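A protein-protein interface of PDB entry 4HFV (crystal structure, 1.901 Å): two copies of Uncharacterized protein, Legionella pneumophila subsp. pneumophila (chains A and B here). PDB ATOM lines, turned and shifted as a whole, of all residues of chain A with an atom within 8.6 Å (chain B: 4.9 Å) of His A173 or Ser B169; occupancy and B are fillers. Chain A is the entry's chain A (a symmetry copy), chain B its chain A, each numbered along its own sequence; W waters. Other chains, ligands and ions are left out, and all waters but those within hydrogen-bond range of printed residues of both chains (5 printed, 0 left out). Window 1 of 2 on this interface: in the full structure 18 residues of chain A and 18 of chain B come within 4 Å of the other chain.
The side-chain carboxylate (OD1) of Asp B170 lies within hydrogen-bond range of a ring nitrogen (NE2) of His A173, at 2.8 Å.
NE2 of His B173 is in hydrogen-bond range of OD1 of Asp A170.
A ring nitrogen (ND1) of His A173 lies close to the side-chain hydroxyl (OG) of Ser B169.
ND1 of His B173 sits close to OG of Ser A169, 3.4 Å away.
CD2 of His B173 touches CD2 of His A173, at 3.3 Å.
Leu B166 touches His A177 (CD2 to ND1, 3.4 Å).
Leu B166 touches Ile A180.
Printed residues of chain B within 4 Å of Ser A169: His B173 (3.1 Å).
Of the printed residues of chain B, Asp A170 touches His B173.
Printed residues of chain B within 4 Å of His A173: Ser B169, Asp B170 and His B173.
Of the printed residues of chain B, Ile A180 touches Leu B166 (3.6 Å).
Of the printed residues of chain A, Leu B166 touches His A177 (3.4 Å) and Ile A180 (3.6 Å).
Of chain A, only His A173 (3.1 Å) comes within 4 Å of Ser B169.
Printed residues of chain A within 4 Å of His B173: Ser A169, Asp A170 and His A173.
Hydrophobic or aromatic side chains of chain B within 4 Å of the printed part of chain A: Leu B166 and His B173.
Hydrophobic or aromatic side chains of chain A that line the printed part of chain B: His A173, His A177 and Ile A180.
Among the printed residues, no Asp or Glu carboxylate lies within 4 Å of a Lys or Arg side-chain nitrogen of the other chain.
Ser A169 touches His B173, and with the chains exchanged His A173 touches Ser B169.
Asp A170 touches His B173, and with the chains exchanged His A173 touches Asp B170.
His B173 touches its own counterpart, His A173.
Of the 7 pairs that touch across the chains among the printed residues, 5 have their exchanged pair printed and touching as well.
Water W4 lies within hydrogen-bond range of ND1 of His A177, OD1 of Asp B170 and O of Leu B166.
Water W3 bridges NE2 of His B173 and OD1 of Asp A170.
Water W2 bridges a ring nitrogen (NE2) of His A173 (2.9 Å) and the side-chain carboxylate (OD1) of Asp B170 (3.2 Å).
Water W5 lies within hydrogen-bond range of the side-chain hydroxyl (OG) of Ser B169 (2.9 Å), the backbone carbonyl oxygen (O) of His A173 (2.9 Å) and the backbone NH (N) of His A177 (3.2 Å).
Water W1 bridges the side-chain hydroxyl (OG) of Ser A169 (2.9 Å) and the backbone carbonyl oxygen (O) of His B173 (2.9 Å).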
ATOM      1  N   LEU A 123      -5.285   3.686  -1.400  1.00  0.00           N
ATOM      2  CA  LEU A 123      -3.999   4.115  -0.887  1.00  0.00           C
ATOM      3  C   LEU A 123      -2.956   3.150  -1.369  1.00  0.00           C
ATOM      4  O   LEU A 123      -1.851   3.562  -1.766  1.00  0.00           O
ATOM      5  CB  LEU A 123      -3.985   4.112   0.631  1.00  0.00           C
ATOM      6  CG  LEU A 123      -4.704   5.311   1.246  1.00  0.00           C
ATOM      7  CD1 LEU A 123      -4.695   5.251   2.760  1.00  0.00           C
ATOM      8  CD2 LEU A 123      -4.049   6.594   0.757  1.00  0.00           C
ATOM      9  N   ALA A 124      -3.294   1.864  -1.305  1.00  0.00           N
ATOM     10  CA  ALA A 124      -2.369   0.855  -1.801  1.00  0.00           C
ATOM     11  C   ALA A 124      -2.024   1.154  -3.267  1.00  0.00           C
ATOM     12  O   ALA A 124      -0.865   1.151  -3.637  1.00  0.00           O
ATOM     13  CB  ALA A 124      -2.917  -0.559  -1.653  1.00  0.00           C
ATOM     14  N   TYR A 127       0.116   4.666  -3.377  1.00  0.00           N
ATOM     15  CA  TYR A 127       1.479   4.604  -2.882  1.00  0.00           C
ATOM     16  C   TYR A 127       2.330   3.635  -3.710  1.00  0.00           C
ATOM     17  O   TYR A 127       3.541   3.838  -3.862  1.00  0.00           O
ATOM     18  CB  TYR A 127       1.554   4.159  -1.426  1.00  0.00           C
ATOM     19  CG  TYR A 127       0.994   5.150  -0.422  1.00  0.00           C
ATOM     20  CD1 TYR A 127       1.044   6.516  -0.645  1.00  0.00           C
ATOM     21  CD2 TYR A 127       0.428   4.696   0.770  1.00  0.00           C
ATOM     22  CE1 TYR A 127       0.531   7.402   0.283  1.00  0.00           C
ATOM     23  CE2 TYR A 127      -0.077   5.565   1.702  1.00  0.00           C
ATOM     24  CZ  TYR A 127      -0.016   6.924   1.451  1.00  0.00           C
ATOM     25  OH  TYR A 127      -0.510   7.806   2.387  1.00  0.00           O
ATOM     26  N   SER A 128       1.716   2.586  -4.222  1.00  0.00           N
ATOM     27  CA  SER A 128       2.448   1.682  -5.085  1.00  0.00           C
ATOM     28  C   SER A 128       2.909   2.424  -6.350  1.00  0.00           C
ATOM     29  O   SER A 128       4.076   2.325  -6.769  1.00  0.00           O
ATOM     30  CB  SER A 128       1.595   0.445  -5.400  1.00  0.00           C
ATOM     31  OG  SER A 128       2.275  -0.439  -6.249  1.00  0.00           O
ATOM     32  N   GLU A 131       5.708   4.828  -5.307  1.00  0.00           N
ATOM     33  CA  GLU A 131       6.946   4.057  -5.139  1.00  0.00           C
ATOM     34  C   GLU A 131       7.567   3.599  -6.471  1.00  0.00           C
ATOM     35  O   GLU A 131       8.777   3.752  -6.664  1.00  0.00           O
ATOM     36  CB  GLU A 131       6.730   2.867  -4.230  1.00  0.00           C
ATOM     37  CG  GLU A 131       8.017   2.125  -3.904  1.00  0.00           C
ATOM     38  CD  GLU A 131       7.792   0.673  -3.712  1.00  0.00           C
ATOM     39  OE1 GLU A 131       6.729   0.327  -3.143  1.00  0.00           O
ATOM     40  OE2 GLU A 131       8.674  -0.114  -4.114  1.00  0.00           O
ATOM     41  N   LEU A 166      11.396   3.012   0.634  1.00  0.00           N
ATOM     42  CA  LEU A 166      11.189   2.029   1.696  1.00  0.00           C
ATOM     43  C   LEU A 166       9.912   2.294   2.475  1.00  0.00           C
ATOM     44  O   LEU A 166       9.129   1.379   2.729  1.00  0.00           O
ATOM     45  CB  LEU A 166      12.376   2.038   2.671  1.00  0.00           C
ATOM     46  CG  LEU A 166      13.709   1.591   2.037  1.00  0.00           C
ATOM     47  CD1 LEU A 166      14.867   2.002   2.878  1.00  0.00           C
ATOM     48  CD2 LEU A 166      13.730   0.076   1.802  1.00  0.00           C
ATOM     49  N   GLU A 167       9.686   3.558   2.833  1.00  0.00           N
ATOM     50  CA  GLU A 167       8.502   3.895   3.604  1.00  0.00           C
ATOM     51  C   GLU A 167       7.232   3.593   2.788  1.00  0.00           C
ATOM     52  O   GLU A 167       6.298   2.984   3.294  1.00  0.00           O
ATOM     53  CB  GLU A 167       8.529   5.356   4.030  1.00  0.00           C
ATOM     54  CG  GLU A 167       7.189   5.851   4.610  1.00  0.00           C
ATOM     55  CD  GLU A 167       6.824   5.237   5.933  1.00  0.00           C
ATOM     56  OE1 GLU A 167       7.740   4.946   6.743  1.00  0.00           O
ATOM     57  OE2 GLU A 167       5.610   5.036   6.160  1.00  0.00           O
ATOM     58  N   LEU A 168       7.210   4.010   1.526  1.00  0.00           N
ATOM     59  CA  LEU A 168       6.070   3.782   0.655  1.00  0.00           C
ATOM     60  C   LEU A 168       5.836   2.281   0.493  1.00  0.00           C
ATOM     61  O   LEU A 168       4.696   1.788   0.516  1.00  0.00           O
ATOM     62  CB  LEU A 168       6.287   4.462  -0.701  1.00  0.00           C
ATOM     63  CG  LEU A 168       6.117   6.014  -0.645  1.00  0.00           C
ATOM     64  CD1 LEU A 168       6.615   6.617  -1.911  1.00  0.00           C
ATOM     65  CD2 LEU A 168       4.646   6.351  -0.460  1.00  0.00           C
ATOM     66  N   SER A 169       6.931   1.553   0.362  1.00  0.00           N
ATOM     67  CA  SER A 169       6.842   0.116   0.271  1.00  0.00           C
ATOM     68  C   SER A 169       6.280  -0.484   1.562  1.00  0.00           C
ATOM     69  O   SER A 169       5.421  -1.366   1.527  1.00  0.00           O
ATOM     70  CB  SER A 169       8.227  -0.435  -0.072  1.00  0.00           C
ATOM     71  OG  SER A 169       8.287  -1.772   0.230  1.00  0.00           O
ATOM     72  N   ASP A 170       6.686   0.045   2.710  1.00  0.00           N
ATOM     73  CA  ASP A 170       6.130  -0.457   3.948  1.00  0.00           C
ATOM     74  C   ASP A 170       4.628  -0.203   4.035  1.00  0.00           C
ATOM     75  O   ASP A 170       3.868  -1.065   4.494  1.00  0.00           O
ATOM     76  CB  ASP A 170       6.800   0.170   5.163  1.00  0.00           C
ATOM     77  CG  ASP A 170       8.246  -0.220   5.312  1.00  0.00           C
ATOM     78  OD1 ASP A 170       8.651  -1.250   4.735  1.00  0.00           O
ATOM     79  OD2 ASP A 170       8.966   0.492   6.047  1.00  0.00           O
ATOM     80  N   ARG A 171       4.181   0.992   3.646  1.00  0.00           N
ATOM     81  CA  ARG A 171       2.763   1.292   3.760  1.00  0.00           C
ATOM     82  C   ARG A 171       1.923   0.419   2.843  1.00  0.00           C
ATOM     83  O   ARG A 171       0.860  -0.079   3.237  1.00  0.00           O
ATOM     84  CB  ARG A 171       2.506   2.776   3.469  1.00  0.00           C
ATOM     85  CG  ARG A 171       3.169   3.687   4.446  1.00  0.00           C
ATOM     86  CD  ARG A 171       2.872   5.179   4.082  1.00  0.00           C
ATOM     87  NE  ARG A 171       3.499   6.065   5.055  1.00  0.00           N
ATOM     88  CZ  ARG A 171       2.992   7.210   5.476  1.00  0.00           C
ATOM     89  NH1 ARG A 171       1.812   7.625   5.023  1.00  0.00           N
ATOM     90  NH2 ARG A 171       3.661   7.923   6.365  1.00  0.00           N
ATOM     91  N   VAL A 172       2.384   0.261   1.607  1.00  0.00           N
ATOM     92  CA  VAL A 172       1.744  -0.638   0.665  1.00  0.00           C
ATOM     93  C   VAL A 172       1.673  -2.054   1.260  1.00  0.00           C
ATOM     94  O   VAL A 172       0.604  -2.672   1.245  1.00  0.00           O
ATOM     95  CB  VAL A 172       2.509  -0.676  -0.692  1.00  0.00           C
ATOM     96  CG1 VAL A 172       2.019  -1.796  -1.603  1.00  0.00           C
ATOM     97  CG2 VAL A 172       2.392   0.637  -1.399  1.00  0.00           C
ATOM     98  N   HIS A 173       2.791  -2.549   1.800  1.00  0.00           N
ATOM     99  CA  HIS A 173       2.823  -3.910   2.348  1.00  0.00           C
ATOM    100  C   HIS A 173       1.749  -4.070   3.464  1.00  0.00           C
ATOM    101  O   HIS A 173       1.040  -5.090   3.537  1.00  0.00           O
ATOM    102  CB  HIS A 173       4.186  -4.234   2.927  1.00  0.00           C
ATOM    103  CG  HIS A 173       4.263  -5.606   3.512  1.00  0.00           C
ATOM    104  ND1 HIS A 173       3.930  -6.735   2.803  1.00  0.00           N
ATOM    105  CD2 HIS A 173       4.636  -6.030   4.744  1.00  0.00           C
ATOM    106  CE1 HIS A 173       4.097  -7.796   3.569  1.00  0.00           C
ATOM    107  NE2 HIS A 173       4.503  -7.391   4.759  1.00  0.00           N
ATOM    108  N   LYS A 174       1.659  -3.072   4.340  1.00  0.00           N
ATOM    109  CA  LYS A 174       0.729  -3.084   5.477  1.00  0.00           C
ATOM    110  C   LYS A 174      -0.710  -3.003   4.959  1.00  0.00           C
ATOM    111  O   LYS A 174      -1.588  -3.765   5.395  1.00  0.00           O
ATOM    112  CB  LYS A 174       1.040  -1.927   6.434  1.00  0.00           C
ATOM    113  CG  LYS A 174       0.114  -1.859   7.675  1.00  0.00           C
ATOM    114  CD  LYS A 174       0.708  -0.970   8.752  1.00  0.00           C
ATOM    115  CE  LYS A 174       0.037  -1.173  10.116  1.00  0.00           C
ATOM    116  NZ  LYS A 174      -1.327  -0.578  10.155  1.00  0.00           N
ATOM    117  N   LEU A 175      -0.934  -2.130   3.976  1.00  0.00           N
ATOM    118  CA  LEU A 175      -2.255  -2.002   3.373  1.00  0.00           C
ATOM    119  C   LEU A 175      -2.716  -3.306   2.708  1.00  0.00           C
ATOM    120  O   LEU A 175      -3.865  -3.767   2.948  1.00  0.00           O
ATOM    121  CB  LEU A 175      -2.308  -0.791   2.414  1.00  0.00           C
ATOM    122  CG  LEU A 175      -2.257   0.603   3.068  1.00  0.00           C
ATOM    123  CD1 LEU A 175      -1.867   1.606   2.012  1.00  0.00           C
ATOM    124  CD2 LEU A 175      -3.589   0.978   3.683  1.00  0.00           C
ATOM    125  N   ARG A 176      -1.834  -3.953   1.942  1.00  0.00           N
ATOM    126  CA  ARG A 176      -2.165  -5.228   1.325  1.00  0.00           C
ATOM    127  C   ARG A 176      -2.433  -6.306   2.365  1.00  0.00           C
ATOM    128  O   ARG A 176      -3.369  -7.102   2.206  1.00  0.00           O
ATOM    129  CB  ARG A 176      -1.076  -5.667   0.334  1.00  0.00           C
ATOM    130  CG  ARG A 176      -1.175  -4.879  -0.927  1.00  0.00           C
ATOM    131  CD  ARG A 176      -0.161  -5.209  -1.963  1.00  0.00           C
ATOM    132  NE  ARG A 176      -0.280  -4.285  -3.101  1.00  0.00           N
ATOM    133  CZ  ARG A 176       0.675  -4.131  -4.022  1.00  0.00           C
ATOM    134  NH1 ARG A 176       1.781  -4.853  -3.948  1.00  0.00           N
ATOM    135  NH2 ARG A 176       0.524  -3.274  -5.020  1.00  0.00           N
ATOM    136  N   HIS A 177      -1.662  -6.286   3.456  1.00  0.00           N
ATOM    137  CA  HIS A 177      -1.922  -7.178   4.590  1.00  0.00           C
ATOM    138  C   HIS A 177      -3.350  -6.975   5.110  1.00  0.00           C
ATOM    139  O   HIS A 177      -4.109  -7.935   5.306  1.00  0.00           O
ATOM    140  CB  HIS A 177      -0.871  -6.936   5.676  1.00  0.00           C
ATOM    141  CG  HIS A 177      -0.967  -7.862   6.847  1.00  0.00           C
ATOM    142  ND1 HIS A 177      -0.137  -8.951   7.000  1.00  0.00           N
ATOM    143  CD2 HIS A 177      -1.779  -7.851   7.930  1.00  0.00           C
ATOM    144  CE1 HIS A 177      -0.443  -9.581   8.122  1.00  0.00           C
ATOM    145  NE2 HIS A 177      -1.438  -8.938   8.704  1.00  0.00           N
ATOM    146  N   GLU A 178      -3.723  -5.714   5.319  1.00  0.00           N
ATOM    147  CA  GLU A 178      -5.020  -5.414   5.923  1.00  0.00           C
ATOM    148  C   GLU A 178      -6.172  -5.809   5.018  1.00  0.00           C
ATOM    149  O   GLU A 178      -7.206  -6.277   5.490  1.00  0.00           O
ATOM    150  CB  GLU A 178      -5.114  -3.935   6.296  1.00  0.00           C
ATOM    151  CG  GLU A 178      -4.098  -3.523   7.326  1.00  0.00           C
ATOM    152  CD  GLU A 178      -4.129  -2.031   7.623  1.00  0.00           C
ATOM    153  OE1 GLU A 178      -4.980  -1.322   7.037  1.00  0.00           O
ATOM    154  OE2 GLU A 178      -3.301  -1.573   8.450  1.00  0.00           O
ATOM    155  N   ILE A 179      -5.985  -5.626   3.721  1.00  0.00           N
ATOM    156  CA  ILE A 179      -6.987  -6.013   2.729  1.00  0.00           C
ATOM    157  C   ILE A 179      -7.252  -7.510   2.749  1.00  0.00           C
ATOM    158  O   ILE A 179      -8.406  -7.980   2.678  1.00  0.00           O
ATOM    159  CB  ILE A 179      -6.537  -5.560   1.326  1.00  0.00           C
ATOM    160  CG1 ILE A 179      -6.724  -4.031   1.203  1.00  0.00           C
ATOM    161  CG2 ILE A 179      -7.320  -6.250   0.216  1.00  0.00           C
ATOM    162  CD1 ILE A 179      -6.011  -3.446  -0.002  1.00  0.00           C
ATOM    163  N   ILE A 180      -6.167  -8.260   2.822  1.00  0.00           N
ATOM    164  CA  ILE A 180      -6.265  -9.729   2.987  1.00  0.00           C
ATOM    165  C   ILE A 180      -7.010 -10.098   4.251  1.00  0.00           C
ATOM    166  O   ILE A 180      -7.938 -10.922   4.231  1.00  0.00           O
ATOM    167  CB  ILE A 180      -4.870 -10.361   2.974  1.00  0.00           C
ATOM    168  CG1 ILE A 180      -4.364 -10.450   1.534  1.00  0.00           C
ATOM    169  CG2 ILE A 180      -4.886 -11.797   3.549  1.00  0.00           C
ATOM    170  CD1 ILE A 180      -2.849 -10.552   1.431  1.00  0.00           C
ATOM    171  N   GLU B 131       3.476 -16.877  -3.901  1.00  0.00           N
ATOM    172  CA  GLU B 131       2.362 -16.074  -3.382  1.00  0.00           C
ATOM    173  C   GLU B 131       1.308 -15.727  -4.449  1.00  0.00           C
ATOM    174  O   GLU B 131       0.110 -15.877  -4.194  1.00  0.00           O
ATOM    175  CB  GLU B 131       2.863 -14.811  -2.715  1.00  0.00           C
ATOM    176  CG  GLU B 131       1.758 -14.022  -2.029  1.00  0.00           C
ATOM    177  CD  GLU B 131       2.012 -12.563  -2.057  1.00  0.00           C
ATOM    178  OE1 GLU B 131       3.202 -12.184  -1.928  1.00  0.00           O
ATOM    179  OE2 GLU B 131       1.033 -11.800  -2.196  1.00  0.00           O
ATOM    180  N   ASP B 164      -0.207 -18.658   4.742  1.00  0.00           N
ATOM    181  CA  ASP B 164       0.922 -18.808   3.833  1.00  0.00           C
ATOM    182  C   ASP B 164       1.095 -17.619   2.865  1.00  0.00           C
ATOM    183  O   ASP B 164       2.214 -17.148   2.628  1.00  0.00           O
ATOM    184  CB  ASP B 164       0.787 -20.143   3.058  1.00  0.00           C
ATOM    185  CG  ASP B 164       1.725 -21.215   3.567  1.00  0.00           C
ATOM    186  OD1 ASP B 164       2.339 -21.071   4.661  1.00  0.00           O
ATOM    187  OD2 ASP B 164       1.797 -22.244   2.864  1.00  0.00           O
ATOM    188  N   ILE B 165       0.000 -17.110   2.316  1.00  0.00           N
ATOM    189  CA  ILE B 165       0.072 -15.898   1.484  1.00  0.00           C
ATOM    190  C   ILE B 165       0.662 -14.699   2.239  1.00  0.00           C
ATOM    191  O   ILE B 165       1.574 -14.041   1.729  1.00  0.00           O
ATOM    192  CB  ILE B 165      -1.283 -15.581   0.900  1.00  0.00           C
ATOM    193  CG1 ILE B 165      -1.595 -16.613  -0.185  1.00  0.00           C
ATOM    194  CG2 ILE B 165      -1.321 -14.131   0.285  1.00  0.00           C
ATOM    195  CD1 ILE B 165      -3.078 -16.777  -0.484  1.00  0.00           C
ATOM    196  N   LEU B 166       0.188 -14.445   3.463  1.00  0.00           N
ATOM    197  CA  LEU B 166       0.736 -13.375   4.293  1.00  0.00           C
ATOM    198  C   LEU B 166       2.209 -13.590   4.599  1.00  0.00           C
ATOM    199  O   LEU B 166       3.016 -12.669   4.481  1.00  0.00           O
ATOM    200  CB  LEU B 166      -0.035 -13.278   5.618  1.00  0.00           C
ATOM    201  CG  LEU B 166      -1.513 -12.867   5.451  1.00  0.00           C
ATOM    202  CD1 LEU B 166      -2.299 -13.184   6.676  1.00  0.00           C
ATOM    203  CD2 LEU B 166      -1.639 -11.380   5.103  1.00  0.00           C
ATOM    204  N   GLU B 167       2.566 -14.820   4.967  1.00  0.00           N
ATOM    205  CA  GLU B 167       3.949 -15.107   5.303  1.00  0.00           C
ATOM    206  C   GLU B 167       4.851 -14.899   4.072  1.00  0.00           C
ATOM    207  O   GLU B 167       5.892 -14.262   4.164  1.00  0.00           O
ATOM    208  CB  GLU B 167       4.097 -16.523   5.840  1.00  0.00           C
ATOM    209  CG  GLU B 167       5.563 -16.985   5.958  1.00  0.00           C
ATOM    210  CD  GLU B 167       6.356 -16.262   7.010  1.00  0.00           C
ATOM    211  OE1 GLU B 167       5.776 -15.885   8.060  1.00  0.00           O
ATOM    212  OE2 GLU B 167       7.570 -16.061   6.781  1.00  0.00           O
ATOM    213  N   LEU B 168       4.438 -15.427   2.925  1.00  0.00           N
ATOM    214  CA  LEU B 168       5.199 -15.297   1.694  1.00  0.00           C
ATOM    215  C   LEU B 168       5.337 -13.820   1.327  1.00  0.00           C
ATOM    216  O   LEU B 168       6.405 -13.345   0.907  1.00  0.00           O
ATOM    217  CB  LEU B 168       4.534 -16.091   0.565  1.00  0.00           C
ATOM    218  CG  LEU B 168       4.738 -17.635   0.697  1.00  0.00           C
ATOM    219  CD1 LEU B 168       3.839 -18.340  -0.257  1.00  0.00           C
ATOM    220  CD2 LEU B 168       6.186 -17.977   0.387  1.00  0.00           C
ATOM    221  N   SER B 169       4.254 -13.089   1.521  1.00  0.00           N
ATOM    222  CA  SER B 169       4.283 -11.668   1.278  1.00  0.00           C
ATOM    223  C   SER B 169       5.250 -10.964   2.232  1.00  0.00           C
ATOM    224  O   SER B 169       6.028 -10.102   1.821  1.00  0.00           O
ATOM    225  CB  SER B 169       2.856 -11.127   1.391  1.00  0.00           C
ATOM    226  OG  SER B 169       2.884  -9.768   1.574  1.00  0.00           O
ATOM    227  N   ASP B 170       5.278 -11.381   3.493  1.00  0.00           N
ATOM    228  CA  ASP B 170       6.222 -10.780   4.408  1.00  0.00           C
ATOM    229  C   ASP B 170       7.664 -11.049   3.989  1.00  0.00           C
ATOM    230  O   ASP B 170       8.523 -10.162   4.074  1.00  0.00           O
ATOM    231  CB  ASP B 170       6.028 -11.285   5.832  1.00  0.00           C
ATOM    232  CG  ASP B 170       4.719 -10.860   6.440  1.00  0.00           C
ATOM    233  OD1 ASP B 170       4.122  -9.879   5.951  1.00  0.00           O
ATOM    234  OD2 ASP B 170       4.312 -11.492   7.441  1.00  0.00           O
ATOM    235  N   ARG B 171       7.967 -12.281   3.576  1.00  0.00           N
ATOM    236  CA  ARG B 171       9.340 -12.592   3.215  1.00  0.00           C
ATOM    237  C   ARG B 171       9.794 -11.819   1.989  1.00  0.00           C
ATOM    238  O   ARG B 171      10.920 -11.305   1.941  1.00  0.00           O
ATOM    239  CB  ARG B 171       9.504 -14.100   2.987  1.00  0.00           C
ATOM    240  CG  ARG B 171       9.237 -14.910   4.211  1.00  0.00           C
ATOM    241  CD  ARG B 171       9.413 -16.433   3.901  1.00  0.00           C
ATOM    242  NE  ARG B 171       9.179 -17.219   5.106  1.00  0.00           N
ATOM    243  CZ  ARG B 171       9.820 -18.329   5.424  1.00  0.00           C
ATOM    244  NH1 ARG B 171      10.774 -18.802   4.628  1.00  0.00           N
ATOM    245  NH2 ARG B 171       9.514 -18.949   6.551  1.00  0.00           N
ATOM    246  N   VAL B 172       8.928 -11.764   0.982  1.00  0.00           N
ATOM    247  CA  VAL B 172       9.186 -10.963  -0.200  1.00  0.00           C
ATOM    248  C   VAL B 172       9.436  -9.501   0.204  1.00  0.00           C
ATOM    249  O   VAL B 172      10.423  -8.905  -0.238  1.00  0.00           O
ATOM    250  CB  VAL B 172       7.994 -11.035  -1.202  1.00  0.00           C
ATOM    251  CG1 VAL B 172       8.118 -10.008  -2.324  1.00  0.00           C
ATOM    252  CG2 VAL B 172       7.878 -12.407  -1.786  1.00  0.00           C
ATOM    253  N   HIS B 173       8.569  -8.942   1.053  1.00  0.00           N
ATOM    254  CA  HIS B 173       8.708  -7.537   1.454  1.00  0.00           C
ATOM    255  C   HIS B 173      10.101  -7.295   2.106  1.00  0.00           C
ATOM    256  O   HIS B 173      10.774  -6.285   1.836  1.00  0.00           O
ATOM    257  CB  HIS B 173       7.627  -7.141   2.441  1.00  0.00           C
ATOM    258  CG  HIS B 173       7.737  -5.721   2.891  1.00  0.00           C
ATOM    259  ND1 HIS B 173       7.784  -4.665   2.012  1.00  0.00           N
ATOM    260  CD2 HIS B 173       7.811  -5.182   4.133  1.00  0.00           C
ATOM    261  CE1 HIS B 173       7.877  -3.537   2.691  1.00  0.00           C
ATOM    262  NE2 HIS B 173       7.918  -3.828   3.978  1.00  0.00           N
HETATM  263  O   HOH W   1      10.480  -3.575   0.807  1.00  0.00           O
HETATM  264  O   HOH W   2       6.029  -7.626   7.186  1.00  0.00           O
HETATM  265  O   HOH W   3       7.330  -3.353   6.754  1.00  0.00           O
HETATM  266  O   HOH W   4       1.494  -9.636   4.939  1.00  0.00           O
HETATM  267  O   HOH W   5       1.001  -7.885   2.716  1.00  0.00           O
